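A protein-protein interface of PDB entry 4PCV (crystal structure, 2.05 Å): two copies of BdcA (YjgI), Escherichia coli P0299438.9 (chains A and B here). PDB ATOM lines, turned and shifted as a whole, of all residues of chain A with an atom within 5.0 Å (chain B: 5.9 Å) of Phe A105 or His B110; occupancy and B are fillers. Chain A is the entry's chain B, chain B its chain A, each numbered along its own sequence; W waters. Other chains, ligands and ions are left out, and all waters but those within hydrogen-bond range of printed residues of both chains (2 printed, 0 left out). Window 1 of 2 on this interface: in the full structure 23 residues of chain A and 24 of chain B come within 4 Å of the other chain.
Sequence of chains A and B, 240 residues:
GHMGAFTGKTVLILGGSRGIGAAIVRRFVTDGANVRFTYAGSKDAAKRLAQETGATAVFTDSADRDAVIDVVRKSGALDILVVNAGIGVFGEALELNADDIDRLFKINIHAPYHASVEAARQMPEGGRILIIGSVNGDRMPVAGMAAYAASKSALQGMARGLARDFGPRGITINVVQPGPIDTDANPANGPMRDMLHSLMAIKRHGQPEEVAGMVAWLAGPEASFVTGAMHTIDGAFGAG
O of Lys B106 sits at hydrogen-bond distance from N of Ala B111 (2.8 Å).
O of Phe B105 is in hydrogen-bond range of N of His B110, at 3.2 Å.
O of Phe A105 lies within hydrogen-bond range of N of His A110.
The side-chain hydroxyl (OG) of Ser A151 lies within hydrogen-bond range of the backbone carbonyl oxygen (O) of Ala A147.
Among the printed residues, pairs that only touch across the chains: Ile A101 with Tyr B113, Ile A101 with His B114, Phe A105 with His B110, Lys A106 with Lys B106, His A110 with Asp B102, His A110 with Phe B105, Ala A147 with Tyr B113 and Ala A150 with Met B158.
Of the 13 printed residues of chain A, 7 touch a printed residue of chain B.
Of the 13 printed residues of chain B, 7 touch a printed residue of chain A.
Hydrophobic or aromatic side chains of chain B within 4 Å of the printed part of chain A: Phe B105, His B110, Tyr B113, His B114 and Met B158.
Among the printed residues, no Asp or Glu carboxylate lies within 4 Å of a Lys or Arg side-chain nitrogen of the other chain.
The side-chain carboxylate of Asp A102 is in hydrogen-bond range of a ring nitrogen (ND1) of His B110.
NE2 of His A110 is in hydrogen-bond range of NE2 of His B110 (2.9 Å).
The side-chain carboxylate of Asp A102 sits at hydrogen-bond distance from a ring nitrogen (NE2) of His B114, at 2.8 Å.
Asp A102 touches His B110, and with the chains exchanged His A110 touches Asp B102.
Phe A105 touches His B110, and with the chains exchanged His A110 touches Phe B105.
Lys A106 touches its own counterpart, Lys B106.
His A110 touches its own counterpart, His B110.
Water W1 lies within hydrogen-bond range of the side-chain hydroxyl (OH) of Tyr B113 (2.6 Å) and the backbone NH (N) of Ala A147 (2.9 Å).
Water W2 bridges OD2 of Asp A102 (3.0 Å) and ND1 of His B110 (3.4 Å).
Of chain B, only His B110 (3.6 Å) comes within 4 Å of Phe A105.
Of the printed residues of chain A, Phe B105 touches His A110 (3.6 Å).
Printed residues of chain A within 4 Å of Lys B106: Lys A106.
Of chain A, only Asp A102 (2.7 Å), Phe A105 (3.6 Å) and His A110 (2.9 Å) come within 4 Å of His B110.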
ATOM      1  N   ILE A 101       9.394 -22.955  -8.464  1.00  0.00           N
ATOM      2  CA  ILE A 101       9.610 -22.133  -7.278  1.00  0.00           C
ATOM      3  C   ILE A 101       8.755 -20.873  -7.353  1.00  0.00           C
ATOM      4  O   ILE A 101       8.061 -20.524  -6.397  1.00  0.00           O
ATOM      5  CB  ILE A 101      11.095 -21.742  -7.120  1.00  0.00           C
ATOM      6  CG1 ILE A 101      11.915 -22.939  -6.638  1.00  0.00           C
ATOM      7  CG2 ILE A 101      11.246 -20.576  -6.145  1.00  0.00           C
ATOM      8  CD1 ILE A 101      11.555 -23.405  -5.244  1.00  0.00           C
ATOM      9  N   ASP A 102       8.803 -20.196  -8.496  1.00  0.00           N
ATOM     10  CA  ASP A 102       7.989 -19.008  -8.709  1.00  0.00           C
ATOM     11  C   ASP A 102       6.504 -19.350  -8.642  1.00  0.00           C
ATOM     12  O   ASP A 102       5.701 -18.552  -8.169  1.00  0.00           O
ATOM     13  CB  ASP A 102       8.319 -18.353 -10.051  1.00  0.00           C
ATOM     14  CG  ASP A 102       9.665 -17.651 -10.043  1.00  0.00           C
ATOM     15  OD1 ASP A 102      10.159 -17.306  -8.948  1.00  0.00           O
ATOM     16  OD2 ASP A 102      10.228 -17.435 -11.136  1.00  0.00           O
ATOM     17  N   ARG A 103       6.146 -20.541  -9.116  1.00  0.00           N
ATOM     18  CA  ARG A 103       4.767 -21.008  -9.028  1.00  0.00           C
ATOM     19  C   ARG A 103       4.356 -21.202  -7.571  1.00  0.00           C
ATOM     20  O   ARG A 103       3.245 -20.842  -7.177  1.00  0.00           O
ATOM     21  CB  ARG A 103       4.587 -22.313  -9.808  1.00  0.00           C
ATOM     22  CG  ARG A 103       3.298 -23.053  -9.487  1.00  0.00           C
ATOM     23  CD  ARG A 103       3.042 -24.177 -10.478  1.00  0.00           C
ATOM     24  NE  ARG A 103       2.728 -23.658 -11.806  1.00  0.00           N
ATOM     25  CZ  ARG A 103       1.503 -23.337 -12.209  1.00  0.00           C
ATOM     26  NH1 ARG A 103       0.473 -23.481 -11.385  1.00  0.00           N
ATOM     27  NH2 ARG A 103       1.308 -22.867 -13.433  1.00  0.00           N
ATOM     28  N   LEU A 104       5.262 -21.768  -6.780  1.00  0.00           N
ATOM     29  CA  LEU A 104       5.038 -21.955  -5.349  1.00  0.00           C
ATOM     30  C   LEU A 104       4.740 -20.619  -4.675  1.00  0.00           C
ATOM     31  O   LEU A 104       3.760 -20.485  -3.942  1.00  0.00           O
ATOM     32  CB  LEU A 104       6.256 -22.629  -4.706  1.00  0.00           C
ATOM     33  CG  LEU A 104       6.215 -23.065  -3.237  1.00  0.00           C
ATOM     34  CD1 LEU A 104       7.178 -24.220  -3.025  1.00  0.00           C
ATOM     35  CD2 LEU A 104       6.564 -21.925  -2.291  1.00  0.00           C
ATOM     36  N   PHE A 105       5.596 -19.634  -4.932  1.00  0.00           N
ATOM     37  CA  PHE A 105       5.437 -18.302  -4.360  1.00  0.00           C
ATOM     38  C   PHE A 105       4.137 -17.640  -4.815  1.00  0.00           C
ATOM     39  O   PHE A 105       3.457 -16.991  -4.026  1.00  0.00           O
ATOM     40  CB  PHE A 105       6.634 -17.418  -4.728  1.00  0.00           C
ATOM     41  CG  PHE A 105       7.887 -17.746  -3.963  1.00  0.00           C
ATOM     42  CD1 PHE A 105       7.815 -18.217  -2.659  1.00  0.00           C
ATOM     43  CD2 PHE A 105       9.136 -17.582  -4.545  1.00  0.00           C
ATOM     44  CE1 PHE A 105       8.965 -18.518  -1.951  1.00  0.00           C
ATOM     45  CE2 PHE A 105      10.289 -17.880  -3.843  1.00  0.00           C
ATOM     46  CZ  PHE A 105      10.205 -18.349  -2.544  1.00  0.00           C
ATOM     47  N   LYS A 106       3.793 -17.812  -6.087  1.00  0.00           N
ATOM     48  CA  LYS A 106       2.569 -17.224  -6.620  1.00  0.00           C
ATOM     49  C   LYS A 106       1.322 -17.852  -5.998  1.00  0.00           C
ATOM     50  O   LYS A 106       0.340 -17.160  -5.724  1.00  0.00           O
ATOM     51  CB  LYS A 106       2.530 -17.361  -8.144  1.00  0.00           C
ATOM     52  CG  LYS A 106       3.468 -16.396  -8.857  1.00  0.00           C
ATOM     53  CD  LYS A 106       3.442 -16.586 -10.361  1.00  0.00           C
ATOM     54  CE  LYS A 106       4.411 -15.632 -11.046  1.00  0.00           C
ATOM     55  NZ  LYS A 106       4.457 -15.844 -12.521  1.00  0.00           N
ATOM     56  N   ILE A 107       1.369 -19.160  -5.769  1.00  0.00           N
ATOM     57  CA  ILE A 107       0.252 -19.868  -5.149  1.00  0.00           C
ATOM     58  C   ILE A 107       0.152 -19.559  -3.655  1.00  0.00           C
ATOM     59  O   ILE A 107      -0.940 -19.338  -3.129  1.00  0.00           O
ATOM     60  CB  ILE A 107       0.379 -21.394  -5.348  1.00  0.00           C
ATOM     61  CG1 ILE A 107       0.191 -21.751  -6.824  1.00  0.00           C
ATOM     62  CG2 ILE A 107      -0.635 -22.139  -4.493  1.00  0.00           C
ATOM     63  CD1 ILE A 107       0.388 -23.220  -7.128  1.00  0.00           C
ATOM     64  N   ASN A 108       1.296 -19.527  -2.977  1.00  0.00           N
ATOM     65  CA  ASN A 108       1.313 -19.377  -1.524  1.00  0.00           C
ATOM     66  C   ASN A 108       1.361 -17.932  -1.030  1.00  0.00           C
ATOM     67  O   ASN A 108       1.008 -17.659   0.116  1.00  0.00           O
ATOM     68  CB  ASN A 108       2.494 -20.149  -0.937  1.00  0.00           C
ATOM     69  CG  ASN A 108       2.249 -21.646  -0.900  1.00  0.00           C
ATOM     70  OD1 ASN A 108       2.343 -22.330  -1.920  1.00  0.00           O
ATOM     71  ND2 ASN A 108       1.936 -22.162   0.281  1.00  0.00           N
ATOM     72  N   ILE A 109       1.793 -17.007  -1.881  1.00  0.00           N
ATOM     73  CA  ILE A 109       1.915 -15.612  -1.462  1.00  0.00           C
ATOM     74  C   ILE A 109       1.104 -14.659  -2.338  1.00  0.00           C
ATOM     75  O   ILE A 109       0.252 -13.926  -1.833  1.00  0.00           O
ATOM     76  CB  ILE A 109       3.388 -15.153  -1.460  1.00  0.00           C
ATOM     77  CG1 ILE A 109       4.244 -16.104  -0.617  1.00  0.00           C
ATOM     78  CG2 ILE A 109       3.499 -13.726  -0.944  1.00  0.00           C
ATOM     79  CD1 ILE A 109       5.717 -15.746  -0.588  1.00  0.00           C
ATOM     80  N   HIS A 110       1.373 -14.668  -3.642  1.00  0.00           N
ATOM     81  CA  HIS A 110       0.705 -13.763  -4.579  1.00  0.00           C
ATOM     82  C   HIS A 110      -0.810 -13.940  -4.586  1.00  0.00           C
ATOM     83  O   HIS A 110      -1.556 -12.973  -4.427  1.00  0.00           O
ATOM     84  CB  HIS A 110       1.237 -13.967  -6.000  1.00  0.00           C
ATOM     85  CG  HIS A 110       2.679 -13.604  -6.171  1.00  0.00           C
ATOM     86  ND1 HIS A 110       3.101 -12.637  -7.057  1.00  0.00           N
ATOM     87  CD2 HIS A 110       3.797 -14.087  -5.580  1.00  0.00           C
ATOM     88  CE1 HIS A 110       4.417 -12.535  -7.001  1.00  0.00           C
ATOM     89  NE2 HIS A 110       4.864 -13.403  -6.113  1.00  0.00           N
ATOM     90  N   ALA A 147      11.786 -22.107   0.757  1.00  0.00           N
ATOM     91  CA  ALA A 147      10.613 -21.603   0.046  1.00  0.00           C
ATOM     92  C   ALA A 147       9.349 -21.751   0.889  1.00  0.00           C
ATOM     93  O   ALA A 147       8.492 -20.867   0.906  1.00  0.00           O
ATOM     94  CB  ALA A 147      10.451 -22.320  -1.287  1.00  0.00           C
ATOM     95  N   ALA A 150       9.503 -19.195   3.889  1.00  0.00           N
ATOM     96  CA  ALA A 150       9.214 -17.843   3.428  1.00  0.00           C
ATOM     97  C   ALA A 150       7.718 -17.639   3.196  1.00  0.00           C
ATOM     98  O   ALA A 150       7.159 -16.615   3.583  1.00  0.00           O
ATOM     99  CB  ALA A 150       9.993 -17.544   2.157  1.00  0.00           C
ATOM    100  N   SER A 151       7.080 -18.620   2.566  1.00  0.00           N
ATOM    101  CA  SER A 151       5.656 -18.538   2.251  1.00  0.00           C
ATOM    102  C   SER A 151       4.787 -18.520   3.508  1.00  0.00           C
ATOM    103  O   SER A 151       3.849 -17.730   3.611  1.00  0.00           O
ATOM    104  CB  SER A 151       5.245 -19.703   1.350  1.00  0.00           C
ATOM    105  OG  SER A 151       5.912 -19.638   0.101  1.00  0.00           O
ATOM    106  N   ASP B 102       3.325  -7.062  -7.591  1.00  0.00           N
ATOM    107  CA  ASP B 102       4.051  -8.221  -8.100  1.00  0.00           C
ATOM    108  C   ASP B 102       5.527  -7.912  -8.303  1.00  0.00           C
ATOM    109  O   ASP B 102       6.386  -8.763  -8.071  1.00  0.00           O
ATOM    110  CB  ASP B 102       3.433  -8.706  -9.409  1.00  0.00           C
ATOM    111  CG  ASP B 102       2.158  -9.491  -9.189  1.00  0.00           C
ATOM    112  OD1 ASP B 102       1.606  -9.423  -8.070  1.00  0.00           O
ATOM    113  OD2 ASP B 102       1.712 -10.176 -10.132  1.00  0.00           O
ATOM    114  N   PHE B 105       7.097  -8.056  -4.894  1.00  0.00           N
ATOM    115  CA  PHE B 105       7.309  -9.427  -4.439  1.00  0.00           C
ATOM    116  C   PHE B 105       8.518 -10.061  -5.120  1.00  0.00           C
ATOM    117  O   PHE B 105       9.282 -10.790  -4.490  1.00  0.00           O
ATOM    118  CB  PHE B 105       6.062 -10.278  -4.691  1.00  0.00           C
ATOM    119  CG  PHE B 105       4.942 -10.009  -3.725  1.00  0.00           C
ATOM    120  CD1 PHE B 105       5.207  -9.538  -2.449  1.00  0.00           C
ATOM    121  CD2 PHE B 105       3.625 -10.231  -4.090  1.00  0.00           C
ATOM    122  CE1 PHE B 105       4.182  -9.293  -1.558  1.00  0.00           C
ATOM    123  CE2 PHE B 105       2.594  -9.988  -3.203  1.00  0.00           C
ATOM    124  CZ  PHE B 105       2.872  -9.517  -1.935  1.00  0.00           C
ATOM    125  N   LYS B 106       8.689  -9.775  -6.406  1.00  0.00           N
ATOM    126  CA  LYS B 106       9.783 -10.356  -7.177  1.00  0.00           C
ATOM    127  C   LYS B 106      11.147  -9.856  -6.711  1.00  0.00           C
ATOM    128  O   LYS B 106      12.134 -10.590  -6.766  1.00  0.00           O
ATOM    129  CB  LYS B 106       9.595 -10.062  -8.666  1.00  0.00           C
ATOM    130  CG  LYS B 106       8.600 -10.988  -9.348  1.00  0.00           C
ATOM    131  CD  LYS B 106       8.319 -10.560 -10.776  1.00  0.00           C
ATOM    132  CE  LYS B 106       7.607 -11.664 -11.542  1.00  0.00           C
ATOM    133  NZ  LYS B 106       6.448 -12.206 -10.780  1.00  0.00           N
ATOM    134  N   ILE B 107      11.199  -8.612  -6.246  1.00  0.00           N
ATOM    135  CA  ILE B 107      12.455  -8.019  -5.803  1.00  0.00           C
ATOM    136  C   ILE B 107      12.745  -8.353  -4.343  1.00  0.00           C
ATOM    137  O   ILE B 107      13.892  -8.584  -3.965  1.00  0.00           O
ATOM    138  CB  ILE B 107      12.448  -6.487  -5.979  1.00  0.00           C
ATOM    139  CG1 ILE B 107      12.126  -6.118  -7.426  1.00  0.00           C
ATOM    140  CG2 ILE B 107      13.790  -5.898  -5.585  1.00  0.00           C
ATOM    141  CD1 ILE B 107      13.122  -6.653  -8.423  1.00  0.00           C
ATOM    142  N   ASN B 108      11.697  -8.385  -3.527  1.00  0.00           N
ATOM    143  CA  ASN B 108      11.852  -8.639  -2.099  1.00  0.00           C
ATOM    144  C   ASN B 108      11.943 -10.120  -1.755  1.00  0.00           C
ATOM    145  O   ASN B 108      12.567 -10.493  -0.764  1.00  0.00           O
ATOM    146  CB  ASN B 108      10.691  -8.011  -1.324  1.00  0.00           C
ATOM    147  CG  ASN B 108      11.125  -6.841  -0.463  1.00  0.00           C
ATOM    148  OD1 ASN B 108      12.205  -6.852   0.130  1.00  0.00           O
ATOM    149  ND2 ASN B 108      10.278  -5.821  -0.388  1.00  0.00           N
ATOM    150  N   ILE B 109      11.316 -10.966  -2.567  1.00  0.00           N
ATOM    151  CA  ILE B 109      11.203 -12.382  -2.226  1.00  0.00           C
ATOM    152  C   ILE B 109      11.841 -13.299  -3.266  1.00  0.00           C
ATOM    153  O   ILE B 109      12.708 -14.108  -2.937  1.00  0.00           O
ATOM    154  CB  ILE B 109       9.729 -12.794  -2.048  1.00  0.00           C
ATOM    155  CG1 ILE B 109       9.029 -11.856  -1.062  1.00  0.00           C
ATOM    156  CG2 ILE B 109       9.629 -14.242  -1.592  1.00  0.00           C
ATOM    157  CD1 ILE B 109       7.552 -12.147  -0.884  1.00  0.00           C
ATOM    158  N   HIS B 110      11.400 -13.174  -4.515  1.00  0.00           N
ATOM    159  CA  HIS B 110      11.870 -14.043  -5.589  1.00  0.00           C
ATOM    160  C   HIS B 110      13.369 -13.905  -5.838  1.00  0.00           C
ATOM    161  O   HIS B 110      14.109 -14.891  -5.784  1.00  0.00           O
ATOM    162  CB  HIS B 110      11.109 -13.751  -6.884  1.00  0.00           C
ATOM    163  CG  HIS B 110       9.670 -14.165  -6.848  1.00  0.00           C
ATOM    164  ND1 HIS B 110       9.165 -15.167  -7.647  1.00  0.00           N
ATOM    165  CD2 HIS B 110       8.629 -13.710  -6.111  1.00  0.00           C
ATOM    166  CE1 HIS B 110       7.875 -15.312  -7.405  1.00  0.00           C
ATOM    167  NE2 HIS B 110       7.525 -14.441  -6.476  1.00  0.00           N
ATOM    168  N   ALA B 111      13.811 -12.682  -6.115  1.00  0.00           N
ATOM    169  CA  ALA B 111      15.214 -12.433  -6.432  1.00  0.00           C
ATOM    170  C   ALA B 111      16.168 -12.866  -5.310  1.00  0.00           C
ATOM    171  O   ALA B 111      17.161 -13.537  -5.589  1.00  0.00           O
ATOM    172  CB  ALA B 111      15.428 -10.954  -6.781  1.00  0.00           C
ATOM    173  N   PRO B 112      15.877 -12.501  -4.042  1.00  0.00           N
ATOM    174  CA  PRO B 112      16.788 -12.983  -2.996  1.00  0.00           C
ATOM    175  C   PRO B 112      16.834 -14.506  -2.888  1.00  0.00           C
ATOM    176  O   PRO B 112      17.897 -15.053  -2.608  1.00  0.00           O
ATOM    177  CB  PRO B 112      16.209 -12.373  -1.714  1.00  0.00           C
ATOM    178  CG  PRO B 112      15.466 -11.179  -2.170  1.00  0.00           C
ATOM    179  CD  PRO B 112      14.870 -11.578  -3.486  1.00  0.00           C
ATOM    180  N   TYR B 113      15.707 -15.178  -3.107  1.00  0.00           N
ATOM    181  CA  TYR B 113      15.686 -16.637  -3.031  1.00  0.00           C
ATOM    182  C   TYR B 113      16.557 -17.269  -4.114  1.00  0.00           C
ATOM    183  O   TYR B 113      17.412 -18.104  -3.824  1.00  0.00           O
ATOM    184  CB  TYR B 113      14.258 -17.178  -3.144  1.00  0.00           C
ATOM    185  CG  TYR B 113      14.200 -18.691  -3.102  1.00  0.00           C
ATOM    186  CD1 TYR B 113      14.240 -19.444  -4.272  1.00  0.00           C
ATOM    187  CD2 TYR B 113      14.124 -19.369  -1.891  1.00  0.00           C
ATOM    188  CE1 TYR B 113      14.201 -20.824  -4.236  1.00  0.00           C
ATOM    189  CE2 TYR B 113      14.080 -20.754  -1.849  1.00  0.00           C
ATOM    190  CZ  TYR B 113      14.119 -21.474  -3.023  1.00  0.00           C
ATOM    191  OH  TYR B 113      14.077 -22.851  -2.989  1.00  0.00           O
ATOM    192  N   HIS B 114      16.322 -16.878  -5.364  1.00  0.00           N
ATOM    193  CA  HIS B 114      17.030 -17.470  -6.495  1.00  0.00           C
ATOM    194  C   HIS B 114      18.528 -17.184  -6.433  1.00  0.00           C
ATOM    195  O   HIS B 114      19.348 -18.073  -6.662  1.00  0.00           O
ATOM    196  CB  HIS B 114      16.451 -16.959  -7.817  1.00  0.00           C
ATOM    197  CG  HIS B 114      15.058 -17.434  -8.088  1.00  0.00           C
ATOM    198  ND1 HIS B 114      14.747 -18.766  -8.260  1.00  0.00           N
ATOM    199  CD2 HIS B 114      13.894 -16.755  -8.220  1.00  0.00           C
ATOM    200  CE1 HIS B 114      13.450 -18.887  -8.484  1.00  0.00           C
ATOM    201  NE2 HIS B 114      12.910 -17.683  -8.466  1.00  0.00           N
ATOM    202  N   ALA B 115      18.879 -15.941  -6.123  1.00  0.00           N
ATOM    203  CA  ALA B 115      20.281 -15.550  -6.028  1.00  0.00           C
ATOM    204  C   ALA B 115      20.995 -16.332  -4.930  1.00  0.00           C
ATOM    205  O   ALA B 115      22.094 -16.844  -5.138  1.00  0.00           O
ATOM    206  CB  ALA B 115      20.401 -14.053  -5.779  1.00  0.00           C
ATOM    207  N   MET B 158      12.470 -16.772   5.204  1.00  0.00           N
ATOM    208  CA  MET B 158      13.438 -17.275   4.235  1.00  0.00           C
ATOM    209  C   MET B 158      14.824 -17.415   4.859  1.00  0.00           C
ATOM    210  O   MET B 158      15.545 -18.373   4.579  1.00  0.00           O
ATOM    211  CB  MET B 158      13.508 -16.356   3.010  1.00  0.00           C
ATOM    212  CG  MET B 158      14.333 -16.921   1.862  1.00  0.00           C
ATOM    213  SD  MET B 158      14.532 -15.766   0.489  1.00  0.00           S
ATOM    214  CE  MET B 158      12.823 -15.407   0.089  1.00  0.00           C
HETATM  215  O   HOH W   1      13.445 -23.954  -0.776  1.00  0.00           O
HETATM  216  O   HOH W   2      11.004 -14.572 -10.503  1.00  0.00           O
